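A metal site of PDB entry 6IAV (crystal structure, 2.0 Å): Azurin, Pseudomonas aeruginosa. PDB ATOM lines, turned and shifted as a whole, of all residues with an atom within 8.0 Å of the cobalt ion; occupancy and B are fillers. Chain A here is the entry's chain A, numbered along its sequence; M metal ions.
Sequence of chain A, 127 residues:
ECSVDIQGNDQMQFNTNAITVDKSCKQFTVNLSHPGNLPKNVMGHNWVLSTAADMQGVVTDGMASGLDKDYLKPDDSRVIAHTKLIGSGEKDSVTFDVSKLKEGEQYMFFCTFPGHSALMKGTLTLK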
ATOM      1  N   GLY A   8      30.717 -18.704  -8.130  1.00  0.00           N
ATOM      2  CA  GLY A   8      30.191 -19.924  -8.797  1.00  0.00           C
ATOM      3  C   GLY A   8      29.773 -19.528 -10.194  1.00  0.00           C
ATOM      4  O   GLY A   8      28.962 -18.600 -10.298  1.00  0.00           O
ATOM      5  N   ASN A   9      30.230 -20.204 -11.227  1.00  0.00           N
ATOM      6  CA  ASN A   9      29.929 -19.791 -12.623  1.00  0.00           C
ATOM      7  C   ASN A   9      28.959 -20.797 -13.274  1.00  0.00           C
ATOM      8  O   ASN A   9      28.363 -21.647 -12.579  1.00  0.00           O
ATOM      9  CB  ASN A   9      31.225 -19.551 -13.396  1.00  0.00           C
ATOM     10  CG  ASN A   9      32.023 -20.830 -13.537  1.00  0.00           C
ATOM     11  OD1 ASN A   9      31.541 -21.922 -13.273  1.00  0.00           O
ATOM     12  ND2 ASN A   9      33.245 -20.741 -13.998  1.00  0.00           N
ATOM     13  N   MET A  12      29.934 -24.622 -13.288  1.00  0.00           N
ATOM     14  CA  MET A  12      29.730 -25.497 -12.120  1.00  0.00           C
ATOM     15  C   MET A  12      31.078 -25.581 -11.400  1.00  0.00           C
ATOM     16  O   MET A  12      31.455 -26.576 -10.871  1.00  0.00           O
ATOM     17  CB  MET A  12      29.197 -26.850 -12.610  1.00  0.00           C
ATOM     18  CG  MET A  12      28.218 -27.482 -11.759  1.00  0.00           C
ATOM     19  SD  MET A  12      27.339 -28.703 -12.851  1.00  0.00           S
ATOM     20  CE  MET A  12      26.398 -27.521 -13.818  1.00  0.00           C
ATOM     21  N   GLN A  13      31.738 -24.458 -11.314  1.00  0.00           N
ATOM     22  CA  GLN A  13      33.054 -24.292 -10.617  1.00  0.00           C
ATOM     23  C   GLN A  13      32.969 -23.224  -9.551  1.00  0.00           C
ATOM     24  O   GLN A  13      32.475 -22.114  -9.883  1.00  0.00           O
ATOM     25  CB  GLN A  13      34.165 -23.864 -11.643  1.00  0.00           C
ATOM     26  CG  GLN A  13      34.271 -24.808 -12.821  1.00  0.00           C
ATOM     27  CD  GLN A  13      35.141 -24.257 -13.969  1.00  0.00           C
ATOM     28  OE1 GLN A  13      35.338 -23.048 -14.126  1.00  0.00           O
ATOM     29  NE2 GLN A  13      35.629 -25.137 -14.834  1.00  0.00           N
ATOM     30  N   PHE A  14      33.475 -23.499  -8.362  1.00  0.00           N
ATOM     31  CA  PHE A  14      33.829 -22.421  -7.413  1.00  0.00           C
ATOM     32  C   PHE A  14      35.269 -21.944  -7.730  1.00  0.00           C
ATOM     33  O   PHE A  14      35.955 -22.718  -8.141  1.00  0.00           O
ATOM     34  CB  PHE A  14      33.787 -22.990  -6.004  1.00  0.00           C
ATOM     35  CG  PHE A  14      32.428 -23.137  -5.367  1.00  0.00           C
ATOM     36  CD1 PHE A  14      31.494 -22.122  -5.451  1.00  0.00           C
ATOM     37  CD2 PHE A  14      32.123 -24.261  -4.623  1.00  0.00           C
ATOM     38  CE1 PHE A  14      30.233 -22.231  -4.838  1.00  0.00           C
ATOM     39  CE2 PHE A  14      30.844 -24.397  -4.019  1.00  0.00           C
ATOM     40  CZ  PHE A  14      29.971 -23.314  -4.042  1.00  0.00           C
ATOM     41  N   LEU A  32      29.534 -14.656  -1.756  1.00  0.00           N
ATOM     42  CA  LEU A  32      29.370 -15.507  -2.934  1.00  0.00           C
ATOM     43  C   LEU A  32      28.768 -14.619  -4.008  1.00  0.00           C
ATOM     44  O   LEU A  32      27.706 -13.934  -3.739  1.00  0.00           O
ATOM     45  CB  LEU A  32      28.376 -16.673  -2.556  1.00  0.00           C
ATOM     46  CG  LEU A  32      28.016 -17.628  -3.708  1.00  0.00           C
ATOM     47  CD1 LEU A  32      29.199 -18.540  -4.167  1.00  0.00           C
ATOM     48  CD2 LEU A  32      26.915 -18.543  -3.411  1.00  0.00           C
ATOM     49  N   HIS A  34      27.524 -14.822  -8.509  1.00  0.00           N
ATOM     50  CA  HIS A  34      27.303 -15.593  -9.751  1.00  0.00           C
ATOM     51  C   HIS A  34      27.676 -14.742 -10.976  1.00  0.00           C
ATOM     52  O   HIS A  34      26.814 -13.987 -11.398  1.00  0.00           O
ATOM     53  CB  HIS A  34      25.832 -16.026  -9.785  1.00  0.00           C
ATOM     54  CG  HIS A  34      25.556 -17.175 -10.710  1.00  0.00           C
ATOM     55  ND1 HIS A  34      26.247 -17.327 -11.966  1.00  0.00           N
ATOM     56  CD2 HIS A  34      24.694 -18.264 -10.556  1.00  0.00           C
ATOM     57  CE1 HIS A  34      25.821 -18.428 -12.517  1.00  0.00           C
ATOM     58  NE2 HIS A  34      24.838 -19.051 -11.664  1.00  0.00           N
ATOM     59  N   LYS A  40      18.709 -18.846 -11.925  1.00  0.00           N
ATOM     60  CA  LYS A  40      18.755 -19.594 -10.638  1.00  0.00           C
ATOM     61  C   LYS A  40      18.141 -20.992 -10.795  1.00  0.00           C
ATOM     62  O   LYS A  40      18.741 -21.927 -10.294  1.00  0.00           O
ATOM     63  CB  LYS A  40      18.024 -18.745  -9.622  1.00  0.00           C
ATOM     64  CG  LYS A  40      18.211 -19.160  -8.193  1.00  0.00           C
ATOM     65  CD  LYS A  40      17.418 -18.323  -7.193  1.00  0.00           C
ATOM     66  CE  LYS A  40      15.931 -18.149  -7.415  1.00  0.00           C
ATOM     67  NZ  LYS A  40      15.567 -16.947  -6.642  1.00  0.00           N
ATOM     68  N   VAL A  42      18.151 -22.939 -13.186  1.00  0.00           N
ATOM     69  CA  VAL A  42      18.922 -23.741 -14.186  1.00  0.00           C
ATOM     70  C   VAL A  42      20.359 -23.979 -13.640  1.00  0.00           C
ATOM     71  O   VAL A  42      20.857 -25.122 -13.787  1.00  0.00           O
ATOM     72  CB  VAL A  42      18.860 -22.972 -15.549  1.00  0.00           C
ATOM     73  CG1 VAL A  42      20.216 -22.792 -16.237  1.00  0.00           C
ATOM     74  CG2 VAL A  42      17.784 -23.495 -16.461  1.00  0.00           C
ATOM     75  N   MET A  43      21.030 -22.929 -13.123  1.00  0.00           N
ATOM     76  CA  MET A  43      22.439 -22.990 -12.671  1.00  0.00           C
ATOM     77  C   MET A  43      22.561 -22.391 -11.257  1.00  0.00           C
ATOM     78  O   MET A  43      23.539 -21.612 -10.963  1.00  0.00           O
ATOM     79  CB  MET A  43      23.313 -22.192 -13.670  1.00  0.00           C
ATOM     80  CG  MET A  43      24.814 -22.426 -13.552  1.00  0.00           C
ATOM     81  SD  MET A  43      25.241 -24.186 -13.486  1.00  0.00           S
ATOM     82  CE  MET A  43      25.338 -24.529 -15.250  1.00  0.00           C
ATOM     83  N   GLY A  44      21.646 -22.735 -10.366  1.00  0.00           N
ATOM     84  CA  GLY A  44      21.648 -22.154  -9.012  1.00  0.00           C
ATOM     85  C   GLY A  44      22.861 -22.526  -8.172  1.00  0.00           C
ATOM     86  O   GLY A  44      23.382 -23.692  -8.272  1.00  0.00           O
ATOM     87  N   HIS A  45      23.394 -21.527  -7.455  1.00  0.00           N
ATOM     88  CA  HIS A  45      24.520 -21.800  -6.536  1.00  0.00           C
ATOM     89  C   HIS A  45      24.215 -21.211  -5.174  1.00  0.00           C
ATOM     90  O   HIS A  45      23.643 -20.142  -5.090  1.00  0.00           O
ATOM     91  CB  HIS A  45      25.879 -21.269  -7.046  1.00  0.00           C
ATOM     92  CG  HIS A  45      26.265 -21.686  -8.419  1.00  0.00           C
ATOM     93  ND1 HIS A  45      26.208 -22.939  -8.813  1.00  0.00           N
ATOM     94  CD2 HIS A  45      26.808 -20.915  -9.451  1.00  0.00           C
ATOM     95  CE1 HIS A  45      26.635 -23.025 -10.084  1.00  0.00           C
ATOM     96  NE2 HIS A  45      27.034 -21.734 -10.552  1.00  0.00           N
ATOM     97  N   ASN A  46      24.643 -21.966  -4.183  1.00  0.00           N
ATOM     98  CA  ASN A  46      24.730 -21.625  -2.785  1.00  0.00           C
ATOM     99  C   ASN A  46      26.073 -22.130  -2.284  1.00  0.00           C
ATOM    100  O   ASN A  46      26.731 -22.884  -2.936  1.00  0.00           O
ATOM    101  CB  ASN A  46      23.494 -22.128  -2.019  1.00  0.00           C
ATOM    102  CG  ASN A  46      23.264 -23.618  -2.061  1.00  0.00           C
ATOM    103  OD1 ASN A  46      24.181 -24.272  -2.402  1.00  0.00           O
ATOM    104  ND2 ASN A  46      22.132 -24.122  -1.617  1.00  0.00           N
ATOM    105  N   TRP A  47      26.394 -21.783  -1.089  1.00  0.00           N
ATOM    106  CA  TRP A  47      27.562 -22.121  -0.244  1.00  0.00           C
ATOM    107  C   TRP A  47      26.933 -22.661   1.027  1.00  0.00           C
ATOM    108  O   TRP A  47      26.543 -21.813   1.738  1.00  0.00           O
ATOM    109  CB  TRP A  47      28.388 -20.863   0.058  1.00  0.00           C
ATOM    110  CG  TRP A  47      29.798 -21.129   0.527  1.00  0.00           C
ATOM    111  CD1 TRP A  47      30.889 -21.535  -0.119  1.00  0.00           C
ATOM    112  CD2 TRP A  47      30.107 -21.272   1.932  1.00  0.00           C
ATOM    113  NE1 TRP A  47      31.910 -21.781   0.774  1.00  0.00           N
ATOM    114  CE2 TRP A  47      31.485 -21.531   2.017  1.00  0.00           C
ATOM    115  CE3 TRP A  47      29.408 -20.891   3.051  1.00  0.00           C
ATOM    116  CZ2 TRP A  47      32.101 -21.678   3.252  1.00  0.00           C
ATOM    117  CZ3 TRP A  47      30.036 -20.882   4.264  1.00  0.00           C
ATOM    118  CH2 TRP A  47      31.339 -21.415   4.377  1.00  0.00           C
ATOM    119  N   LEU A  85      20.517 -19.264  -2.318  1.00  0.00           N
ATOM    120  CA  LEU A  85      20.626 -19.823  -3.654  1.00  0.00           C
ATOM    121  C   LEU A  85      20.535 -18.621  -4.577  1.00  0.00           C
ATOM    122  O   LEU A  85      19.514 -17.969  -4.520  1.00  0.00           O
ATOM    123  CB  LEU A  85      19.488 -20.801  -4.026  1.00  0.00           C
ATOM    124  CG  LEU A  85      19.778 -21.501  -5.369  1.00  0.00           C
ATOM    125  CD1 LEU A  85      20.823 -22.613  -5.183  1.00  0.00           C
ATOM    126  CD2 LEU A  85      18.547 -22.007  -6.122  1.00  0.00           C
ATOM    127  N   ILE A  86      21.451 -18.456  -5.466  1.00  0.00           N
ATOM    128  CA  ILE A  86      21.496 -17.303  -6.397  1.00  0.00           C
ATOM    129  C   ILE A  86      21.697 -17.788  -7.829  1.00  0.00           C
ATOM    130  O   ILE A  86      22.304 -18.848  -8.025  1.00  0.00           O
ATOM    131  CB  ILE A  86      22.605 -16.318  -5.967  1.00  0.00           C
ATOM    132  CG1 ILE A  86      23.991 -16.892  -6.144  1.00  0.00           C
ATOM    133  CG2 ILE A  86      22.367 -15.887  -4.516  1.00  0.00           C
ATOM    134  CD1 ILE A  86      25.036 -15.723  -5.905  1.00  0.00           C
ATOM    135  N   PHE A 110      30.087 -26.722  -0.165  1.00  0.00           N
ATOM    136  CA  PHE A 110      29.450 -27.335  -1.346  1.00  0.00           C
ATOM    137  C   PHE A 110      28.209 -26.546  -1.721  1.00  0.00           C
ATOM    138  O   PHE A 110      27.626 -25.769  -1.027  1.00  0.00           O
ATOM    139  CB  PHE A 110      29.119 -28.806  -1.083  1.00  0.00           C
ATOM    140  CG  PHE A 110      28.400 -29.057   0.215  1.00  0.00           C
ATOM    141  CD1 PHE A 110      27.049 -29.028   0.253  1.00  0.00           C
ATOM    142  CD2 PHE A 110      29.083 -29.367   1.367  1.00  0.00           C
ATOM    143  CE1 PHE A 110      26.382 -29.305   1.430  1.00  0.00           C
ATOM    144  CE2 PHE A 110      28.396 -29.791   2.509  1.00  0.00           C
ATOM    145  CZ  PHE A 110      27.053 -29.754   2.529  1.00  0.00           C
ATOM    146  N   CYS A 111      27.843 -26.778  -2.918  1.00  0.00           N
ATOM    147  CA  CYS A 111      26.544 -26.326  -3.495  1.00  0.00           C
ATOM    148  C   CYS A 111      25.578 -27.458  -3.400  1.00  0.00           C
ATOM    149  O   CYS A 111      25.941 -28.612  -3.807  1.00  0.00           O
ATOM    150  CB  CYS A 111      26.644 -26.114  -4.989  1.00  0.00           C
ATOM    151  SG  CYS A 111      25.243 -25.152  -5.597  1.00  0.00           S
ATOM    152  N   THR A 112      24.339 -27.173  -3.044  1.00  0.00           N
ATOM    153  CA  THR A 112      23.344 -28.287  -2.991  1.00  0.00           C
ATOM    154  C   THR A 112      22.417 -28.218  -4.145  1.00  0.00           C
ATOM    155  O   THR A 112      21.373 -28.894  -4.094  1.00  0.00           O
ATOM    156  CB  THR A 112      22.571 -28.223  -1.656  1.00  0.00           C
ATOM    157  OG1 THR A 112      21.912 -26.992  -1.574  1.00  0.00           O
ATOM    158  CG2 THR A 112      23.425 -28.398  -0.428  1.00  0.00           C
ATOM    159  N   PHE A 113      22.566 -27.346  -5.113  1.00  0.00           N
ATOM    160  CA  PHE A 113      21.709 -27.362  -6.299  1.00  0.00           C
ATOM    161  C   PHE A 113      21.954 -28.730  -6.924  1.00  0.00           C
ATOM    162  O   PHE A 113      23.107 -29.247  -6.828  1.00  0.00           O
ATOM    163  CB  PHE A 113      22.024 -26.228  -7.260  1.00  0.00           C
ATOM    164  CG  PHE A 113      21.099 -26.130  -8.443  1.00  0.00           C
ATOM    165  CD1 PHE A 113      21.377 -26.856  -9.602  1.00  0.00           C
ATOM    166  CD2 PHE A 113      20.029 -25.205  -8.448  1.00  0.00           C
ATOM    167  CE1 PHE A 113      20.545 -26.700 -10.709  1.00  0.00           C
ATOM    168  CE2 PHE A 113      19.257 -25.001  -9.601  1.00  0.00           C
ATOM    169  CZ  PHE A 113      19.483 -25.794 -10.718  1.00  0.00           C
ATOM    170  N   PRO A 114      20.929 -29.441  -7.462  1.00  0.00           N
ATOM    171  CA  PRO A 114      21.042 -30.819  -7.955  1.00  0.00           C
ATOM    172  C   PRO A 114      22.195 -31.086  -8.940  1.00  0.00           C
ATOM    173  O   PRO A 114      22.178 -30.524 -10.047  1.00  0.00           O
ATOM    174  CB  PRO A 114      19.706 -31.125  -8.663  1.00  0.00           C
ATOM    175  CG  PRO A 114      18.792 -30.271  -7.825  1.00  0.00           C
ATOM    176  CD  PRO A 114      19.541 -29.023  -7.578  1.00  0.00           C
ATOM    177  N   GLY A 115      23.095 -31.918  -8.403  1.00  0.00           N
ATOM    178  CA  GLY A 115      24.212 -32.648  -9.003  1.00  0.00           C
ATOM    179  C   GLY A 115      25.413 -31.736  -8.952  1.00  0.00           C
ATOM    180  O   GLY A 115      26.397 -32.092  -9.440  1.00  0.00           O
ATOM    181  N   HIS A 116      25.340 -30.578  -8.346  1.00  0.00           N
ATOM    182  CA  HIS A 116      26.427 -29.555  -8.409  1.00  0.00           C
ATOM    183  C   HIS A 116      27.592 -29.975  -7.504  1.00  0.00           C
ATOM    184  O   HIS A 116      28.805 -29.677  -7.916  1.00  0.00           O
ATOM    185  CB  HIS A 116      25.852 -28.182  -8.102  1.00  0.00           C
ATOM    186  CG  HIS A 116      25.330 -27.450  -9.270  1.00  0.00           C
ATOM    187  ND1 HIS A 116      25.105 -26.075  -9.312  1.00  0.00           N
ATOM    188  CD2 HIS A 116      25.004 -27.928 -10.486  1.00  0.00           C
ATOM    189  CE1 HIS A 116      24.426 -25.793 -10.427  1.00  0.00           C
ATOM    190  NE2 HIS A 116      24.362 -26.887 -11.139  1.00  0.00           N
ATOM    191  N   SER A 117      27.314 -30.693  -6.433  1.00  0.00           N
ATOM    192  CA  SER A 117      28.211 -31.063  -5.342  1.00  0.00           C
ATOM    193  C   SER A 117      29.365 -31.929  -5.858  1.00  0.00           C
ATOM    194  O   SER A 117      30.408 -32.002  -5.143  1.00  0.00           O
ATOM    195  CB  SER A 117      27.578 -31.704  -4.121  1.00  0.00           C
ATOM    196  OG  SER A 117      27.174 -32.996  -4.339  1.00  0.00           O
ATOM    197  N   MET A 120      31.346 -28.873  -7.248  1.00  0.00           N
ATOM    198  CA  MET A 120      31.291 -27.630  -6.440  1.00  0.00           C
ATOM    199  C   MET A 120      31.421 -28.010  -4.985  1.00  0.00           C
ATOM    200  O   MET A 120      30.459 -28.121  -4.277  1.00  0.00           O
ATOM    201  CB  MET A 120      30.081 -26.746  -6.735  1.00  0.00           C
ATOM    202  CG  MET A 120      29.854 -26.295  -8.150  1.00  0.00           C
ATOM    203  SD  MET A 120      28.508 -25.135  -8.397  1.00  0.00           S
ATOM    204  CE  MET A 120      29.191 -23.492  -7.953  1.00  0.00           C
HETATM  205 CO    CO M   1      25.412 -24.760  -7.882  1.00  0.00          CO
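SD of Met 43 sits close to NE2 of His 116 (3.7 Å).
O of Asn 9 is in hydrogen-bond range of NE2 of His 45, 2.4 Å away.
ND1 of His 45 lies close to SD of Met 120.
A ring nitrogen (ND1) of His 116 sits close to the side-chain sulfur (SD) of Met 120, at 3.6 Å.
The backbone NH (N) of Phe 113 sits close to the side-chain sulfur (SG) of Cys 111.
The backbone carbonyl oxygen (O) of His 45 lies within hydrogen-bond range of the backbone NH (N) of Ile 86 (2.8 Å).
N of Cys 111 sits at hydrogen-bond distance from O of Met 120, 3.2 Å away.
The side-chain sulfur of Cys 111 lies close to the side-chain amide oxygen of Asn 46, at 3.5 Å.
ND1 of His 116 binds the cobalt ion (2.0 Å).
The cobalt ion is bound by a ring nitrogen (ND1) of His 45 (2.2 Å).
The side-chain sulfur (SG) of Cys 111 is bound to the cobalt ion, 2.3 Å away.
The cobalt ion is bound by O of Gly 44, at 2.3 Å.
Merely in contact with the cobalt ion: Met 120 and Phe 113.
Of the 25 residues printed, 6 come within 4 Å of the cobalt ion.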
